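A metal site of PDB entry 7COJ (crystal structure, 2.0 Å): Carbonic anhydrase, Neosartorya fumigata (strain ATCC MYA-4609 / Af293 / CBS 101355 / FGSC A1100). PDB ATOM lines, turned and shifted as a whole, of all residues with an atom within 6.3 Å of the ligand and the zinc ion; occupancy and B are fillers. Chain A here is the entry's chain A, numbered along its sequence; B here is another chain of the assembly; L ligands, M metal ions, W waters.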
ATOM      1  N   CYS A 119      24.396 -11.048  -5.508  1.00  0.00           N
ATOM      2  CA  CYS A 119      23.589 -11.034  -6.726  1.00  0.00           C
ATOM      3  C   CYS A 119      23.529 -12.454  -7.304  1.00  0.00           C
ATOM      4  O   CYS A 119      24.526 -13.205  -7.216  1.00  0.00           O
ATOM      5  CB  CYS A 119      24.097 -10.006  -7.716  1.00  0.00           C
ATOM      6  SG  CYS A 119      22.946  -9.833  -9.030  1.00  0.00           S
ATOM      7  N   SER A 120      22.414 -12.776  -7.934  1.00  0.00           N
ATOM      8  CA  SER A 120      22.196 -14.028  -8.722  1.00  0.00           C
ATOM      9  C   SER A 120      23.113 -14.056  -9.931  1.00  0.00           C
ATOM     10  O   SER A 120      23.295 -15.127 -10.536  1.00  0.00           O
ATOM     11  CB  SER A 120      20.757 -14.103  -9.103  1.00  0.00           C
ATOM     12  OG  SER A 120      19.960 -14.280  -7.946  1.00  0.00           O
ATOM     13  N   ASP A 121      23.641 -12.900 -10.354  1.00  0.00           N
ATOM     14  CA  ASP A 121      24.504 -12.781 -11.550  1.00  0.00           C
ATOM     15  C   ASP A 121      25.469 -13.978 -11.582  1.00  0.00           C
ATOM     16  O   ASP A 121      26.168 -14.252 -10.574  1.00  0.00           O
ATOM     17  CB  ASP A 121      25.277 -11.434 -11.551  1.00  0.00           C
ATOM     18  CG  ASP A 121      25.979 -11.120 -12.847  1.00  0.00           C
ATOM     19  OD1 ASP A 121      26.922 -11.883 -13.249  1.00  0.00           O
ATOM     20  OD2 ASP A 121      25.618 -10.105 -13.429  1.00  0.00           O
ATOM     21  N   SER A 122      25.521 -14.668 -12.733  1.00  0.00           N
ATOM     22  CA  SER A 122      26.291 -15.912 -12.936  1.00  0.00           C
ATOM     23  C   SER A 122      27.778 -15.656 -12.694  1.00  0.00           C
ATOM     24  O   SER A 122      28.490 -16.640 -12.419  1.00  0.00           O
ATOM     25  CB  SER A 122      26.061 -16.464 -14.293  1.00  0.00           C
ATOM     26  OG  SER A 122      26.518 -15.565 -15.307  1.00  0.00           O
ATOM     27  N   ARG A 123      28.229 -14.416 -12.807  1.00  0.00           N
ATOM     28  CA  ARG A 123      29.654 -14.073 -12.635  1.00  0.00           C
ATOM     29  C   ARG A 123      30.039 -13.942 -11.151  1.00  0.00           C
ATOM     30  O   ARG A 123      31.240 -13.771 -10.927  1.00  0.00           O
ATOM     31  CB  ARG A 123      29.993 -12.789 -13.406  1.00  0.00           C
ATOM     32  CG  ARG A 123      29.689 -12.913 -14.895  1.00  0.00           C
ATOM     33  CD  ARG A 123      29.695 -11.604 -15.667  1.00  0.00           C
ATOM     34  NE  ARG A 123      28.597 -10.765 -15.269  1.00  0.00           N
ATOM     35  CZ  ARG A 123      28.372  -9.527 -15.701  1.00  0.00           C
ATOM     36  NH1 ARG A 123      29.105  -9.011 -16.692  1.00  0.00           N
ATOM     37  NH2 ARG A 123      27.325  -8.848 -15.238  1.00  0.00           N
ATOM     38  N   CYS A 124      29.125 -14.068 -10.168  1.00  0.00           N
ATOM     39  CA  CYS A 124      29.420 -13.877  -8.716  1.00  0.00           C
ATOM     40  C   CYS A 124      29.152 -15.127  -7.882  1.00  0.00           C
ATOM     41  O   CYS A 124      28.444 -15.052  -6.872  1.00  0.00           O
ATOM     42  CB  CYS A 124      28.585 -12.727  -8.181  1.00  0.00           C
ATOM     43  SG  CYS A 124      28.666 -11.231  -9.206  1.00  0.00           S
ATOM     44  N   ASN A 142      20.012 -13.086  -5.007  1.00  0.00           N
ATOM     45  CA  ASN A 142      18.758 -12.575  -5.588  1.00  0.00           C
ATOM     46  C   ASN A 142      19.156 -11.512  -6.604  1.00  0.00           C
ATOM     47  O   ASN A 142      20.367 -11.199  -6.709  1.00  0.00           O
ATOM     48  CB  ASN A 142      17.771 -12.169  -4.489  1.00  0.00           C
ATOM     49  CG  ASN A 142      18.209 -10.942  -3.713  1.00  0.00           C
ATOM     50  OD1 ASN A 142      18.961 -10.131  -4.254  1.00  0.00           O
ATOM     51  ND2 ASN A 142      17.692 -10.794  -2.487  1.00  0.00           N
ATOM     52  N   ILE A 143      18.195 -10.978  -7.355  1.00  0.00           N
ATOM     53  CA  ILE A 143      18.504  -9.941  -8.369  1.00  0.00           C
ATOM     54  C   ILE A 143      19.011  -8.694  -7.635  1.00  0.00           C
ATOM     55  O   ILE A 143      18.224  -8.093  -6.858  1.00  0.00           O
ATOM     56  CB  ILE A 143      17.270  -9.605  -9.223  1.00  0.00           C
ATOM     57  CG1 ILE A 143      16.746 -10.823 -10.012  1.00  0.00           C
ATOM     58  CG2 ILE A 143      17.568  -8.434 -10.138  1.00  0.00           C
ATOM     59  CD1 ILE A 143      17.726 -11.335 -10.999  1.00  0.00           C
ATOM     60  N   ALA A 144      20.252  -8.299  -7.910  1.00  0.00           N
ATOM     61  CA  ALA A 144      20.881  -7.056  -7.430  1.00  0.00           C
ATOM     62  C   ALA A 144      21.039  -7.048  -5.904  1.00  0.00           C
ATOM     63  O   ALA A 144      21.199  -5.945  -5.328  1.00  0.00           O
ATOM     64  CB  ALA A 144      20.094  -5.867  -7.904  1.00  0.00           C
ATOM     65  N   ASN A 145      21.117  -8.216  -5.273  1.00  0.00           N
ATOM     66  CA  ASN A 145      21.445  -8.321  -3.823  1.00  0.00           C
ATOM     67  C   ASN A 145      20.616  -7.293  -3.057  1.00  0.00           C
ATOM     68  O   ASN A 145      21.159  -6.603  -2.195  1.00  0.00           O
ATOM     69  CB  ASN A 145      22.960  -8.184  -3.557  1.00  0.00           C
ATOM     70  CG  ASN A 145      23.650  -7.017  -4.235  1.00  0.00           C
ATOM     71  OD1 ASN A 145      24.057  -7.111  -5.401  1.00  0.00           O
ATOM     72  ND2 ASN A 145      23.807  -5.907  -3.493  1.00  0.00           N
ATOM     73  N   HIS A 175      28.062  -5.821  -7.145  1.00  0.00           N
ATOM     74  CA  HIS A 175      29.117  -6.084  -8.158  1.00  0.00           C
ATOM     75  C   HIS A 175      29.057  -5.004  -9.239  1.00  0.00           C
ATOM     76  O   HIS A 175      28.020  -4.327  -9.371  1.00  0.00           O
ATOM     77  CB  HIS A 175      29.022  -7.529  -8.687  1.00  0.00           C
ATOM     78  CG  HIS A 175      27.825  -7.730  -9.532  1.00  0.00           C
ATOM     79  ND1 HIS A 175      27.891  -7.732 -10.930  1.00  0.00           N
ATOM     80  CD2 HIS A 175      26.536  -7.934  -9.194  1.00  0.00           C
ATOM     81  CE1 HIS A 175      26.673  -7.918 -11.412  1.00  0.00           C
ATOM     82  NE2 HIS A 175      25.877  -8.076 -10.373  1.00  0.00           N
ATOM     83  N   LYS A 177      28.916  -3.760 -13.117  1.00  0.00           N
ATOM     84  CA  LYS A 177      28.136  -4.214 -14.302  1.00  0.00           C
ATOM     85  C   LYS A 177      26.895  -5.004 -13.822  1.00  0.00           C
ATOM     86  O   LYS A 177      26.538  -5.977 -14.470  1.00  0.00           O
ATOM     87  CB  LYS A 177      29.032  -5.073 -15.191  1.00  0.00           C
ATOM     88  CG  LYS A 177      30.382  -4.456 -15.550  1.00  0.00           C
ATOM     89  CD  LYS A 177      30.220  -3.263 -16.417  1.00  0.00           C
ATOM     90  CE  LYS A 177      30.059  -3.676 -17.863  1.00  0.00           C
ATOM     91  NZ  LYS A 177      29.100  -2.838 -18.622  1.00  0.00           N
ATOM     92  N   CYS A 178      26.311  -4.628 -12.688  1.00  0.00           N
ATOM     93  CA  CYS A 178      25.036  -5.223 -12.206  1.00  0.00           C
ATOM     94  C   CYS A 178      23.910  -4.648 -13.059  1.00  0.00           C
ATOM     95  O   CYS A 178      23.583  -3.466 -12.892  1.00  0.00           O
ATOM     96  CB  CYS A 178      24.823  -5.022 -10.705  1.00  0.00           C
ATOM     97  SG  CYS A 178      23.328  -5.800 -10.113  1.00  0.00           S
ATOM     98  N   GLY A 179      23.331  -5.488 -13.929  1.00  0.00           N
ATOM     99  CA  GLY A 179      22.244  -5.039 -14.811  1.00  0.00           C
ATOM    100  C   GLY A 179      20.958  -4.781 -14.039  1.00  0.00           C
ATOM    101  O   GLY A 179      20.128  -4.049 -14.543  1.00  0.00           O
ATOM    102  N   GLY A 180      20.780  -5.395 -12.853  1.00  0.00           N
ATOM    103  CA  GLY A 180      19.669  -5.039 -11.961  1.00  0.00           C
ATOM    104  C   GLY A 180      19.744  -3.579 -11.529  1.00  0.00           C
ATOM    105  O   GLY A 180      18.728  -2.838 -11.638  1.00  0.00           O
ATOM    106  N   VAL A 181      20.900  -3.162 -11.045  1.00  0.00           N
ATOM    107  CA  VAL A 181      21.161  -1.735 -10.675  1.00  0.00           C
ATOM    108  C   VAL A 181      20.949  -0.856 -11.921  1.00  0.00           C
ATOM    109  O   VAL A 181      20.260   0.164 -11.822  1.00  0.00           O
ATOM    110  CB  VAL A 181      22.576  -1.597 -10.074  1.00  0.00           C
ATOM    111  CG1 VAL A 181      22.959  -0.130  -9.878  1.00  0.00           C
ATOM    112  CG2 VAL A 181      22.681  -2.369  -8.757  1.00  0.00           C
ATOM    113  N   ALA A 183      19.112  -1.431 -14.599  1.00  0.00           N
ATOM    114  CA  ALA A 183      17.667  -1.410 -14.940  1.00  0.00           C
ATOM    115  C   ALA A 183      16.948  -0.374 -14.068  1.00  0.00           C
ATOM    116  O   ALA A 183      16.052   0.290 -14.581  1.00  0.00           O
ATOM    117  CB  ALA A 183      17.062  -2.786 -14.783  1.00  0.00           C
ATOM    118  N   LYS A 188      12.207   1.635 -18.382  1.00  0.00           N
ATOM    119  CA  LYS A 188      11.520   0.575 -19.177  1.00  0.00           C
ATOM    120  C   LYS A 188      10.709  -0.265 -18.177  1.00  0.00           C
ATOM    121  O   LYS A 188      11.263  -0.593 -17.098  1.00  0.00           O
ATOM    122  CB  LYS A 188      12.555  -0.232 -19.974  1.00  0.00           C
ATOM    123  CG  LYS A 188      13.572   0.577 -20.781  1.00  0.00           C
ATOM    124  CD  LYS A 188      15.018  -0.003 -20.854  1.00  0.00           C
ATOM    125  CE  LYS A 188      15.925   0.369 -19.675  1.00  0.00           C
ATOM    126  NZ  LYS A 188      15.783  -0.530 -18.500  1.00  0.00           N
ATOM    127  N   LEU A 190       9.281  -3.560 -16.711  1.00  0.00           N
ATOM    128  CA  LEU A 190       9.976  -4.885 -16.750  1.00  0.00           C
ATOM    129  C   LEU A 190       9.110  -5.961 -16.112  1.00  0.00           C
ATOM    130  O   LEU A 190       9.663  -7.026 -15.709  1.00  0.00           O
ATOM    131  CB  LEU A 190      11.321  -4.718 -16.056  1.00  0.00           C
ATOM    132  CG  LEU A 190      12.316  -3.831 -16.804  1.00  0.00           C
ATOM    133  CD1 LEU A 190      13.388  -3.330 -15.857  1.00  0.00           C
ATOM    134  CD2 LEU A 190      12.873  -4.562 -18.011  1.00  0.00           C
ATOM    135  N   LEU A 193       9.700  -7.730 -12.458  1.00  0.00           N
ATOM    136  CA  LEU A 193      10.983  -7.124 -11.985  1.00  0.00           C
ATOM    137  C   LEU A 193      10.747  -5.721 -11.400  1.00  0.00           C
ATOM    138  O   LEU A 193      11.557  -5.349 -10.542  1.00  0.00           O
ATOM    139  CB  LEU A 193      11.991  -7.092 -13.148  1.00  0.00           C
ATOM    140  CG  LEU A 193      12.658  -8.442 -13.416  1.00  0.00           C
ATOM    141  CD1 LEU A 193      13.198  -8.489 -14.838  1.00  0.00           C
ATOM    142  CD2 LEU A 193      13.769  -8.690 -12.402  1.00  0.00           C
ATOM    143  N   LEU A 197      12.624  -4.231  -7.960  1.00  0.00           N
ATOM    144  CA  LEU A 197      13.699  -3.217  -8.042  1.00  0.00           C
ATOM    145  C   LEU A 197      13.298  -1.916  -7.312  1.00  0.00           C
ATOM    146  O   LEU A 197      14.106  -0.956  -7.315  1.00  0.00           O
ATOM    147  CB  LEU A 197      13.992  -2.954  -9.525  1.00  0.00           C
ATOM    148  CG  LEU A 197      14.603  -4.125 -10.284  1.00  0.00           C
ATOM    149  CD1 LEU A 197      14.702  -3.828 -11.755  1.00  0.00           C
ATOM    150  CD2 LEU A 197      15.957  -4.519  -9.748  1.00  0.00           C
ATOM    151  N   GLN B 110      27.181 -11.473 -19.317  1.00  0.00           N
ATOM    152  CA  GLN B 110      27.038 -12.877 -18.913  1.00  0.00           C
ATOM    153  C   GLN B 110      26.152 -13.576 -19.946  1.00  0.00           C
ATOM    154  O   GLN B 110      25.251 -12.939 -20.485  1.00  0.00           O
ATOM    155  CB  GLN B 110      26.469 -12.939 -17.501  1.00  0.00           C
ATOM    156  CG  GLN B 110      25.076 -12.361 -17.372  1.00  0.00           C
ATOM    157  CD  GLN B 110      24.494 -12.511 -15.998  1.00  0.00           C
ATOM    158  OE1 GLN B 110      24.676 -13.551 -15.358  1.00  0.00           O
ATOM    159  NE2 GLN B 110      23.743 -11.509 -15.561  1.00  0.00           N
ATOM    160  N   PHE B 138      23.458 -19.013 -13.436  1.00  0.00           N
ATOM    161  CA  PHE B 138      22.633 -17.975 -12.801  1.00  0.00           C
ATOM    162  C   PHE B 138      21.992 -18.599 -11.573  1.00  0.00           C
ATOM    163  O   PHE B 138      21.431 -19.700 -11.700  1.00  0.00           O
ATOM    164  CB  PHE B 138      21.626 -17.413 -13.778  1.00  0.00           C
ATOM    165  CG  PHE B 138      21.091 -16.077 -13.338  1.00  0.00           C
ATOM    166  CD1 PHE B 138      21.858 -14.940 -13.475  1.00  0.00           C
ATOM    167  CD2 PHE B 138      19.844 -15.984 -12.757  1.00  0.00           C
ATOM    168  CE1 PHE B 138      21.357 -13.714 -13.070  1.00  0.00           C
ATOM    169  CE2 PHE B 138      19.331 -14.749 -12.380  1.00  0.00           C
ATOM    170  CZ  PHE B 138      20.114 -13.634 -12.492  1.00  0.00           C
ATOM    171  N   PHE B 160      13.869 -12.840 -15.096  1.00  0.00           N
ATOM    172  CA  PHE B 160      15.137 -12.347 -15.680  1.00  0.00           C
ATOM    173  C   PHE B 160      15.886 -13.467 -16.408  1.00  0.00           C
ATOM    174  O   PHE B 160      16.293 -13.292 -17.569  1.00  0.00           O
ATOM    175  CB  PHE B 160      16.018 -11.658 -14.649  1.00  0.00           C
ATOM    176  CG  PHE B 160      17.272 -11.148 -15.290  1.00  0.00           C
ATOM    177  CD1 PHE B 160      17.197 -10.110 -16.215  1.00  0.00           C
ATOM    178  CD2 PHE B 160      18.501 -11.754 -15.065  1.00  0.00           C
ATOM    179  CE1 PHE B 160      18.355  -9.648 -16.838  1.00  0.00           C
ATOM    180  CE2 PHE B 160      19.636 -11.291 -15.697  1.00  0.00           C
ATOM    181  CZ  PHE B 160      19.553 -10.250 -16.611  1.00  0.00           C
ATOM    182  N   HIS B 164      15.137 -12.743 -20.197  1.00  0.00           N
ATOM    183  CA  HIS B 164      16.262 -11.843 -20.603  1.00  0.00           C
ATOM    184  C   HIS B 164      17.529 -12.651 -20.936  1.00  0.00           C
ATOM    185  O   HIS B 164      18.071 -12.477 -22.014  1.00  0.00           O
ATOM    186  CB  HIS B 164      16.508 -10.774 -19.549  1.00  0.00           C
ATOM    187  CG  HIS B 164      15.323  -9.901 -19.301  1.00  0.00           C
ATOM    188  ND1 HIS B 164      15.351  -8.552 -19.586  1.00  0.00           N
ATOM    189  CD2 HIS B 164      14.147 -10.129 -18.689  1.00  0.00           C
ATOM    190  CE1 HIS B 164      14.187  -8.005 -19.264  1.00  0.00           C
ATOM    191  NE2 HIS B 164      13.418  -8.956 -18.709  1.00  0.00           N
ATOM    192  N   LEU B 165      17.999 -13.511 -20.054  1.00  0.00           N
ATOM    193  CA  LEU B 165      19.250 -14.257 -20.311  1.00  0.00           C
ATOM    194  C   LEU B 165      18.964 -15.402 -21.265  1.00  0.00           C
ATOM    195  O   LEU B 165      19.915 -15.880 -21.854  1.00  0.00           O
ATOM    196  CB  LEU B 165      19.857 -14.773 -19.008  1.00  0.00           C
ATOM    197  CG  LEU B 165      20.382 -13.683 -18.072  1.00  0.00           C
ATOM    198  CD1 LEU B 165      20.988 -14.322 -16.836  1.00  0.00           C
ATOM    199  CD2 LEU B 165      21.385 -12.775 -18.765  1.00  0.00           C
HETATM  200  C1  LIG L   1      20.974  -8.579 -13.735  1.00  0.00           C
HETATM  201  C2  LIG L   1      19.344  -7.405 -14.969  1.00  0.00           C
HETATM  202  C3  LIG L   1      17.029  -6.713 -14.953  1.00  0.00           C
HETATM  203  C4  LIG L   1      15.948  -6.117 -15.794  1.00  0.00           C
HETATM  204  N1  LIG L   1      23.273  -8.681 -12.378  1.00  0.00           N
HETATM  205  N2  LIG L   1      20.522  -7.428 -15.562  1.00  0.00           N
HETATM  206  N3  LIG L   1      21.447  -8.174 -14.852  1.00  0.00           N
HETATM  207  N4  LIG L   1      18.253  -6.803 -15.552  1.00  0.00           N
HETATM  208  O1  LIG L   1      21.108  -9.459 -11.419  1.00  0.00           O
HETATM  209  O2  LIG L   1      22.261 -10.705 -13.247  1.00  0.00           O
HETATM  210  O3  LIG L   1      16.863  -7.133 -13.820  1.00  0.00           O
HETATM  211  S1  LIG L   1      21.939  -9.501 -12.574  1.00  0.00           S
HETATM  212  S2  LIG L   1      19.333  -8.209 -13.466  1.00  0.00           S
HETATM  213 ZN    ZN M   1      23.742  -8.125 -10.402  1.00  0.00          ZN
HETATM  214  O   HOH W   1      21.409  -7.589 -18.189  1.00  0.00           O
HETATM  215  O   HOH W   2      18.451  -5.696 -17.958  1.00  0.00           O
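Merely in contact with the zinc ion: Asp 121.
Four residues have an atom within 4 Å of the zinc ion: Cys 119, Asp 121, His 175 and Cys 178.
The nearest printed residue that does not touch the zinc ion is Ala 144 (4.3 Å).
Ile 143 touches the ligand (CG2 to S2, 3.8 Å).
N of Ala 144 touches O1 of the ligand (3.8 Å).
Ala 183 touches the ligand.
Leu 190 touches the ligand.
Leu 193 touches the ligand (CD2 to O3, 3.7 Å).
Phe 138 of chain B touches the ligand (CE1 to O2, 3.1 Å).
CE1 of Phe 160 of chain B touches C2 of the ligand, 3.1 Å away.
Hydrophobic or aromatic side chains within 4 Å of the ligand: Ile 143, His 175, Ala 183, Leu 190, Leu 193, Phe 138 of chain B and Phe 160 of chain B.
14 residues have an atom within 4 Å of the ligand: Cys 119, Asp 121, Ile 143, Ala 144, His 175, Cys 178, Gly 179, Gly 180, Ala 183, Leu 190, Leu 193, Gln 110 of chain B, Phe 138 of chain B and Phe 160 of chain B.
The side-chain amide nitrogen (NE2) of Gln 110 of chain B is in hydrogen-bond range of an oxygen (O2) of the ligand, 2.9 Å away.
The backbone carbonyl oxygen (O) of Gly 179 sits close to a nitrogen (N4) of the ligand.
N of Gly 180 lies close to S2 of the ligand (3.2 Å).
The backbone NH (N) of Gly 179 lies close to a nitrogen (N3) of the ligand, 3.4 Å away.
A nitrogen (N1) of the ligand sits close to the side-chain carboxylate (OD2) of Asp 121 (2.9 Å).
NE2 of Gln 110 of chain B lies within hydrogen-bond range of OD2 of Asp 121.
The side-chain sulfur (SG) of Cys 178 sits close to the backbone NH (N) of Val 181 (3.7 Å).
The side-chain hydroxyl (OG) of Ser 122 lies within hydrogen-bond range of the side-chain amide oxygen (OE1) of Gln 110 of chain B, at 2.7 Å.
O of Phe 160 of chain B lies within hydrogen-bond range of N of Leu 165 of chain B (3.0 Å).
The guanidinium group of Arg 123 lies within salt-bridge range of the side-chain carboxylate of Asp 121 (2.8 Å).
The backbone NH (N) of Ala 144 sits close to the side-chain sulfur (SG) of Cys 119 (3.3 Å).
The side-chain sulfur (SG) of Cys 119 sits close to the backbone carbonyl oxygen (O) of Asn 142 (3.7 Å).
N of Gly 180 sits close to SG of Cys 178.
N1 of the ligand is bound to the zinc ion (2.1 Å).
The zinc ion is bound by NE2 of His 175 (2.1 Å).
The side-chain sulfur (SG) of Cys 119 binds the zinc ion, at 2.3 Å.
SG of Cys 178 binds the zinc ion (2.4 Å).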
